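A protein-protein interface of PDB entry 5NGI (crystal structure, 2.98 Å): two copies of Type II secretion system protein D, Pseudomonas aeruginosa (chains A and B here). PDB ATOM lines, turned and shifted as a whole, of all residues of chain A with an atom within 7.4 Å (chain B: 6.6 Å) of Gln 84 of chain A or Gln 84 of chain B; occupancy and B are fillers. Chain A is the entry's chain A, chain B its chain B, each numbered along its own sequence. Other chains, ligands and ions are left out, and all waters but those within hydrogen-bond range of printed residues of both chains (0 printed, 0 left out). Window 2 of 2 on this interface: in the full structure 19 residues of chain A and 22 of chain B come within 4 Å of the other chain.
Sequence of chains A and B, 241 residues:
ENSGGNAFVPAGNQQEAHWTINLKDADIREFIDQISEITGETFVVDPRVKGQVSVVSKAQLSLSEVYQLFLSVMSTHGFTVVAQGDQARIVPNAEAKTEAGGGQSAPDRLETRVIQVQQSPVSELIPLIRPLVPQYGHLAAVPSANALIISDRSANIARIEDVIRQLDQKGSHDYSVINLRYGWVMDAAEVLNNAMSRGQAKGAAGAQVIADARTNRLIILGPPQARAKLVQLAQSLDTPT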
ATOM      1  N   VAL A  44     -11.045 -11.857  12.396  1.00  0.00           N
ATOM      2  CA  VAL A  44     -10.829 -10.970  13.537  1.00  0.00           C
ATOM      3  C   VAL A  44     -11.520  -9.641  13.242  1.00  0.00           C
ATOM      4  O   VAL A  44     -11.095  -8.897  12.357  1.00  0.00           O
ATOM      5  CB  VAL A  44      -9.323 -10.815  13.909  1.00  0.00           C
ATOM      6  CG1 VAL A  44      -9.133  -9.834  15.065  1.00  0.00           C
ATOM      7  CG2 VAL A  44      -8.692 -12.166  14.244  1.00  0.00           C
ATOM      8  N   ASP A  46     -12.565  -5.842  13.995  1.00  0.00           N
ATOM      9  CA  ASP A  46     -12.106  -4.652  14.708  1.00  0.00           C
ATOM     10  C   ASP A  46     -13.311  -4.135  15.527  1.00  0.00           C
ATOM     11  O   ASP A  46     -14.434  -4.231  15.032  1.00  0.00           O
ATOM     12  CB  ASP A  46     -11.628  -3.577  13.711  1.00  0.00           C
ATOM     13  CG  ASP A  46     -11.263  -2.242  14.343  1.00  0.00           C
ATOM     14  OD1 ASP A  46     -10.125  -2.113  14.844  1.00  0.00           O
ATOM     15  OD2 ASP A  46     -12.133  -1.342  14.378  1.00  0.00           O
ATOM     16  N   VAL A  81     -11.095  -6.836   4.067  1.00  0.00           N
ATOM     17  CA  VAL A  81     -10.437  -7.998   4.675  1.00  0.00           C
ATOM     18  C   VAL A  81      -8.932  -7.978   4.342  1.00  0.00           C
ATOM     19  O   VAL A  81      -8.551  -7.952   3.163  1.00  0.00           O
ATOM     20  CB  VAL A  81     -11.147  -9.324   4.256  1.00  0.00           C
ATOM     21  CG1 VAL A  81     -10.410 -10.557   4.773  1.00  0.00           C
ATOM     22  CG2 VAL A  81     -12.605  -9.342   4.715  1.00  0.00           C
ATOM     23  N   VAL A  82      -8.092  -7.973   5.397  1.00  0.00           N
ATOM     24  CA  VAL A  82      -6.632  -7.940   5.274  1.00  0.00           C
ATOM     25  C   VAL A  82      -6.003  -9.142   5.928  1.00  0.00           C
ATOM     26  O   VAL A  82      -6.516  -9.620   6.938  1.00  0.00           O
ATOM     27  CB  VAL A  82      -5.986  -6.619   5.812  1.00  0.00           C
ATOM     28  CG1 VAL A  82      -6.438  -5.402   5.015  1.00  0.00           C
ATOM     29  CG2 VAL A  82      -6.227  -6.410   7.311  1.00  0.00           C
ATOM     30  N   ALA A  83      -4.874  -9.613   5.387  1.00  0.00           N
ATOM     31  CA  ALA A  83      -4.130 -10.689   6.042  1.00  0.00           C
ATOM     32  C   ALA A  83      -3.088  -9.986   6.932  1.00  0.00           C
ATOM     33  O   ALA A  83      -1.976  -9.662   6.488  1.00  0.00           O
ATOM     34  CB  ALA A  83      -3.471 -11.611   5.024  1.00  0.00           C
ATOM     35  N   GLN A  84      -3.528  -9.634   8.157  1.00  0.00           N
ATOM     36  CA  GLN A  84      -2.736  -8.921   9.163  1.00  0.00           C
ATOM     37  C   GLN A  84      -2.510  -9.837  10.360  1.00  0.00           C
ATOM     38  O   GLN A  84      -3.446 -10.493  10.827  1.00  0.00           O
ATOM     39  CB  GLN A  84      -3.432  -7.599   9.579  1.00  0.00           C
ATOM     40  CG  GLN A  84      -2.490  -6.512  10.110  1.00  0.00           C
ATOM     41  CD  GLN A  84      -3.108  -5.131  10.073  1.00  0.00           C
ATOM     42  OE1 GLN A  84      -3.083  -4.443   9.056  1.00  0.00           O
ATOM     43  NE2 GLN A  84      -3.646  -4.676  11.191  1.00  0.00           N
ATOM     44  N   GLY A  85      -1.254  -9.909  10.796  1.00  0.00           N
ATOM     45  CA  GLY A  85      -0.817 -10.719  11.928  1.00  0.00           C
ATOM     46  C   GLY A  85      -1.022 -12.215  11.773  1.00  0.00           C
ATOM     47  O   GLY A  85      -1.277 -12.902  12.768  1.00  0.00           O
ATOM     48  N   ASP A  86      -0.899 -12.729  10.522  1.00  0.00           N
ATOM     49  CA  ASP A  86      -1.032 -14.144  10.129  1.00  0.00           C
ATOM     50  C   ASP A  86      -2.441 -14.722  10.400  1.00  0.00           C
ATOM     51  O   ASP A  86      -2.583 -15.850  10.904  1.00  0.00           O
ATOM     52  CB  ASP A  86       0.080 -15.021  10.756  1.00  0.00           C
ATOM     53  N   GLN A  87      -3.476 -13.931  10.040  1.00  0.00           N
ATOM     54  CA  GLN A  87      -4.908 -14.250  10.173  1.00  0.00           C
ATOM     55  C   GLN A  87      -5.709 -13.200   9.403  1.00  0.00           C
ATOM     56  O   GLN A  87      -5.169 -12.131   9.101  1.00  0.00           O
ATOM     57  CB  GLN A  87      -5.353 -14.266  11.652  1.00  0.00           C
ATOM     58  N   ALA A  88      -6.988 -13.482   9.076  1.00  0.00           N
ATOM     59  CA  ALA A  88      -7.816 -12.511   8.350  1.00  0.00           C
ATOM     60  C   ALA A  88      -8.523 -11.541   9.309  1.00  0.00           C
ATOM     61  O   ALA A  88      -9.160 -11.970  10.275  1.00  0.00           O
ATOM     62  CB  ALA A  88      -8.809 -13.220   7.453  1.00  0.00           C
ATOM     63  N   ARG A  89      -8.358 -10.229   9.059  1.00  0.00           N
ATOM     64  CA  ARG A  89      -8.885  -9.140   9.883  1.00  0.00           C
ATOM     65  C   ARG A  89      -9.823  -8.234   9.085  1.00  0.00           C
ATOM     66  O   ARG A  89      -9.540  -7.926   7.927  1.00  0.00           O
ATOM     67  CB  ARG A  89      -7.711  -8.321  10.446  1.00  0.00           C
ATOM     68  CG  ARG A  89      -7.947  -7.682  11.802  1.00  0.00           C
ATOM     69  CD  ARG A  89      -6.686  -6.988  12.267  1.00  0.00           C
ATOM     70  NE  ARG A  89      -6.765  -6.578  13.668  1.00  0.00           N
ATOM     71  CZ  ARG A  89      -7.203  -5.395  14.087  1.00  0.00           C
ATOM     72  NH1 ARG A  89      -7.622  -4.487  13.208  1.00  0.00           N
ATOM     73  NH2 ARG A  89      -7.231  -5.109  15.380  1.00  0.00           N
ATOM     74  N   VAL A  91     -11.333  -4.553   8.822  1.00  0.00           N
ATOM     75  CA  VAL A  91     -11.087  -3.133   9.126  1.00  0.00           C
ATOM     76  C   VAL A  91     -11.788  -2.205   8.135  1.00  0.00           C
ATOM     77  O   VAL A  91     -11.965  -2.605   6.986  1.00  0.00           O
ATOM     78  CB  VAL A  91      -9.581  -2.800   9.202  1.00  0.00           C
ATOM     79  CG1 VAL A  91      -9.123  -2.697  10.646  1.00  0.00           C
ATOM     80  CG2 VAL A  91      -8.736  -3.799   8.417  1.00  0.00           C
ATOM     81  N   PRO A  92     -12.154  -0.952   8.507  1.00  0.00           N
ATOM     82  CA  PRO A  92     -12.865  -0.092   7.548  1.00  0.00           C
ATOM     83  C   PRO A  92     -11.996   0.517   6.441  1.00  0.00           C
ATOM     84  O   PRO A  92     -10.886   0.995   6.698  1.00  0.00           O
ATOM     85  CB  PRO A  92     -13.521   0.974   8.437  1.00  0.00           C
ATOM     86  CG  PRO A  92     -13.299   0.519   9.853  1.00  0.00           C
ATOM     87  CD  PRO A  92     -12.061  -0.294   9.822  1.00  0.00           C
ATOM     88  N   VAL B  44       1.188   4.754   6.322  1.00  0.00           N
ATOM     89  CA  VAL B  44       2.021   3.772   7.015  1.00  0.00           C
ATOM     90  C   VAL B  44       2.113   2.568   6.105  1.00  0.00           C
ATOM     91  O   VAL B  44       1.117   1.880   5.881  1.00  0.00           O
ATOM     92  CB  VAL B  44       1.627   3.359   8.463  1.00  0.00           C
ATOM     93  CG1 VAL B  44       2.742   3.692   9.446  1.00  0.00           C
ATOM     94  CG2 VAL B  44       0.296   3.947   8.909  1.00  0.00           C
ATOM     95  N   ASP B  46       3.287  -1.067   5.268  1.00  0.00           N
ATOM     96  CA  ASP B  46       3.607  -2.318   5.959  1.00  0.00           C
ATOM     97  C   ASP B  46       4.924  -2.867   5.393  1.00  0.00           C
ATOM     98  O   ASP B  46       5.162  -2.725   4.188  1.00  0.00           O
ATOM     99  CB  ASP B  46       2.460  -3.339   5.804  1.00  0.00           C
ATOM    100  CG  ASP B  46       2.551  -4.589   6.672  1.00  0.00           C
ATOM    101  OD1 ASP B  46       3.432  -5.432   6.409  1.00  0.00           O
ATOM    102  OD2 ASP B  46       1.678  -4.769   7.554  1.00  0.00           O
ATOM    103  N   ARG B  48       5.934  -5.768   4.461  1.00  0.00           N
ATOM    104  CA  ARG B  48       5.799  -6.720   3.362  1.00  0.00           C
ATOM    105  C   ARG B  48       5.377  -6.048   2.015  1.00  0.00           C
ATOM    106  O   ARG B  48       5.297  -6.748   0.997  1.00  0.00           O
ATOM    107  CB  ARG B  48       4.886  -7.898   3.754  1.00  0.00           C
ATOM    108  CG  ARG B  48       3.454  -7.510   4.041  1.00  0.00           C
ATOM    109  CD  ARG B  48       2.822  -8.372   5.104  1.00  0.00           C
ATOM    110  NE  ARG B  48       1.787  -7.608   5.796  1.00  0.00           N
ATOM    111  CZ  ARG B  48       0.859  -8.131   6.587  1.00  0.00           C
ATOM    112  NH1 ARG B  48       0.812  -9.440   6.794  1.00  0.00           N
ATOM    113  NH2 ARG B  48      -0.039  -7.347   7.170  1.00  0.00           N
ATOM    114  N   VAL B  82      -6.272   1.098   4.788  1.00  0.00           N
ATOM    115  CA  VAL B  82      -7.150   1.001   5.972  1.00  0.00           C
ATOM    116  C   VAL B  82      -6.843   2.088   6.966  1.00  0.00           C
ATOM    117  O   VAL B  82      -5.689   2.479   7.087  1.00  0.00           O
ATOM    118  CB  VAL B  82      -7.201  -0.396   6.645  1.00  0.00           C
ATOM    119  CG1 VAL B  82      -7.819  -1.420   5.718  1.00  0.00           C
ATOM    120  CG2 VAL B  82      -5.828  -0.858   7.119  1.00  0.00           C
ATOM    121  N   ALA B  83      -7.863   2.573   7.684  1.00  0.00           N
ATOM    122  CA  ALA B  83      -7.696   3.648   8.669  1.00  0.00           C
ATOM    123  C   ALA B  83      -7.332   3.117  10.062  1.00  0.00           C
ATOM    124  O   ALA B  83      -8.199   2.612  10.786  1.00  0.00           O
ATOM    125  CB  ALA B  83      -8.955   4.506   8.731  1.00  0.00           C
ATOM    126  N   GLN B  84      -6.039   3.215  10.423  1.00  0.00           N
ATOM    127  CA  GLN B  84      -5.522   2.776  11.719  1.00  0.00           C
ATOM    128  C   GLN B  84      -4.872   3.953  12.431  1.00  0.00           C
ATOM    129  O   GLN B  84      -3.981   4.595  11.866  1.00  0.00           O
ATOM    130  CB  GLN B  84      -4.560   1.575  11.576  1.00  0.00           C
ATOM    131  CG  GLN B  84      -5.286   0.224  11.385  1.00  0.00           C
ATOM    132  CD  GLN B  84      -4.590  -0.988  11.993  1.00  0.00           C
ATOM    133  OE1 GLN B  84      -4.779  -2.130  11.545  1.00  0.00           O
ATOM    134  NE2 GLN B  84      -3.810  -0.787  13.056  1.00  0.00           N
ATOM    135  N   GLY B  85      -5.377   4.258  13.630  1.00  0.00           N
ATOM    136  CA  GLY B  85      -4.907   5.361  14.462  1.00  0.00           C
ATOM    137  C   GLY B  85      -5.014   6.737  13.826  1.00  0.00           C
ATOM    138  O   GLY B  85      -4.129   7.575  14.043  1.00  0.00           O
ATOM    139  N   ASP B  86      -6.107   6.979  13.039  1.00  0.00           N
ATOM    140  CA  ASP B  86      -6.415   8.243  12.335  1.00  0.00           C
ATOM    141  C   ASP B  86      -5.341   8.632  11.290  1.00  0.00           C
ATOM    142  O   ASP B  86      -4.902   9.790  11.204  1.00  0.00           O
ATOM    143  CB  ASP B  86      -6.709   9.392  13.317  1.00  0.00           C
ATOM    144  N   GLN B  87      -4.929   7.626  10.502  1.00  0.00           N
ATOM    145  CA  GLN B  87      -3.968   7.694   9.406  1.00  0.00           C
ATOM    146  C   GLN B  87      -4.142   6.438   8.558  1.00  0.00           C
ATOM    147  O   GLN B  87      -4.616   5.408   9.056  1.00  0.00           O
ATOM    148  CB  GLN B  87      -2.524   7.822   9.921  1.00  0.00           C
ATOM    149  N   ALA B  88      -3.801   6.555   7.269  1.00  0.00           N
ATOM    150  CA  ALA B  88      -3.909   5.501   6.274  1.00  0.00           C
ATOM    151  C   ALA B  88      -2.778   4.490   6.408  1.00  0.00           C
ATOM    152  O   ALA B  88      -1.615   4.870   6.548  1.00  0.00           O
ATOM    153  CB  ALA B  88      -3.896   6.113   4.899  1.00  0.00           C
ATOM    154  N   ARG B  89      -3.133   3.198   6.358  1.00  0.00           N
ATOM    155  CA  ARG B  89      -2.229   2.057   6.479  1.00  0.00           C
ATOM    156  C   ARG B  89      -2.333   1.209   5.206  1.00  0.00           C
ATOM    157  O   ARG B  89      -3.440   0.833   4.820  1.00  0.00           O
ATOM    158  CB  ARG B  89      -2.628   1.222   7.712  1.00  0.00           C
ATOM    159  CG  ARG B  89      -1.469   0.647   8.502  1.00  0.00           C
ATOM    160  CD  ARG B  89      -1.965  -0.438   9.430  1.00  0.00           C
ATOM    161  NE  ARG B  89      -0.914  -0.950  10.310  1.00  0.00           N
ATOM    162  CZ  ARG B  89      -0.093  -1.954  10.010  1.00  0.00           C
ATOM    163  NH1 ARG B  89      -0.171  -2.549   8.824  1.00  0.00           N
ATOM    164  NH2 ARG B  89       0.820  -2.357  10.879  1.00  0.00           N
ATOM    165  N   VAL B  91      -1.752  -2.275   3.568  1.00  0.00           N
ATOM    166  CA  VAL B  91      -1.651  -3.717   3.853  1.00  0.00           C
ATOM    167  C   VAL B  91      -2.168  -4.570   2.686  1.00  0.00           C
ATOM    168  O   VAL B  91      -3.050  -4.110   1.966  1.00  0.00           O
ATOM    169  CB  VAL B  91      -2.369  -4.110   5.161  1.00  0.00           C
ATOM    170  CG1 VAL B  91      -1.371  -4.300   6.283  1.00  0.00           C
ATOM    171  CG2 VAL B  91      -3.457  -3.113   5.545  1.00  0.00           C
ATOM    172  N   PRO B  92      -1.690  -5.820   2.490  1.00  0.00           N
ATOM    173  CA  PRO B  92      -2.168  -6.606   1.340  1.00  0.00           C
ATOM    174  C   PRO B  92      -3.573  -7.190   1.479  1.00  0.00           C
ATOM    175  O   PRO B  92      -3.934  -7.730   2.529  1.00  0.00           O
ATOM    176  CB  PRO B  92      -1.100  -7.696   1.175  1.00  0.00           C
ATOM    177  CG  PRO B  92       0.026  -7.317   2.132  1.00  0.00           C
ATOM    178  CD  PRO B  92      -0.625  -6.540   3.215  1.00  0.00           C
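Of the 13 printed residues of chain B, 7 touch a printed residue of chain A. Hydrophobic or aromatic side chains of chain B that line the printed part of chain A: Val 82 and Val 91. Hydrophobic or aromatic side chains of chain A that line the printed part of chain B: Val 82 and Val 91. Along chain A the printed residues that touch a printed residue of chain B span positions 82 to 92. Among the printed residues, no Asp or Glu carboxylate lies within 4 Å of a Lys or Arg side-chain nitrogen of the other chain.
Of the printed residues of chain B, Val 82 of chain A touches Val 91 and Pro 92. Of the printed residues of chain B, Ala 83 of chain A touches Arg 48 and Pro 92. Gln 84 of chain A touches four residues of chain B. Gln 87 of chain A touches none of the printed residues of chain B. Printed residues of chain B within 4 Å of Val 91 of chain A: Val 82 (3.7 Å). Val 44 of chain B touches none of the printed residues of chain A. Printed residues of chain A within 4 Å of Arg 48 of chain B: Ala 83 and Gln 84. Of the printed residues of chain A, Ala 83 of chain B touches Pro 92 (3.5 Å). The nearest residue of chain B that does not touch Gln 84 of chain A is Val 82 of chain B (4.9 Å). The nearest residue of chain A that does not touch Gln 84 of chain B is Arg 89 of chain A (4.1 Å). The nearest printed residue of chain B that does not touch Pro 92 of chain A is Gln 84 of chain B (6.5 Å).
The side-chain amide oxygen (OE1) of Gln 84 of chain A is in hydrogen-bond range of the guanidinium group (NH1) of Arg 89 of chain B, 3.5 Å away. The guanidinium group (NH1) of Arg 48 of chain B lies within hydrogen-bond range of the backbone carbonyl oxygen (O) of Ala 83 of chain A, 2.8 Å away. The side-chain amide oxygen (OE1) of Gln 84 of chain B sits at hydrogen-bond distance from the side-chain amide nitrogen (NE2) of Gln 84 of chain A (2.8 Å).
Val 82 of chain A touches Pro 92 of chain B, and with the chains exchanged Pro 92 of chain A touches Val 82 of chain B. Gln 84 of chain B touches its own counterpart, Gln 84 of chain A. Gln 84 of chain A touches Arg 89 of chain B, but with the chains exchanged Arg 89 of chain A does not touch Gln 84 of chain B (4.1 Å). Gln 84 of chain A touches Val 91 of chain B, but with the chains exchanged Val 91 of chain A does not touch Gln 84 of chain B (4.5 Å). Positions printed for both chains: 44, 46, 82, 83, 84, 85, 86, 87, 88, 89, 91 and 92.
O of Val 82 of chain A is in hydrogen-bond range of N of Arg 89 of chain A (2.9 Å). The side-chain carboxylate (OD2) of Asp 46 of chain B lies within salt-bridge range of the guanidinium group (NH1) of Arg 89 of chain B, 3.2 Å away. N of Arg 89 of chain B sits at hydrogen-bond distance from O of Val 82 of chain B, 2.8 Å away. The guanidinium group (NE) of Arg 48 of chain B is in salt-bridge range of the side-chain carboxylate (OD1) of Asp 46 of chain B, at 2.8 Å.
CG2 of Val 91 of chain B touches CG1 of Val 82 of chain A, at 3.8 Å. Val 82 of chain A touches Pro 92 of chain B (CA to O, 3.9 Å). O of Pro 92 of chain B touches N of Ala 83 of chain A, at 3.5 Å. NH2 of Arg 48 of chain B touches CA of Gln 84 of chain A (3.7 Å). Gln 84 of chain A touches Val 91 of chain B. Val 82 of chain B touches Val 91 of chain A (CG1 to CG2, 3.7 Å). Pro 92 of chain A touches Val 82 of chain B (O to CA, 3.8 Å). Pro 92 of chain A touches Ala 83 of chain B.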
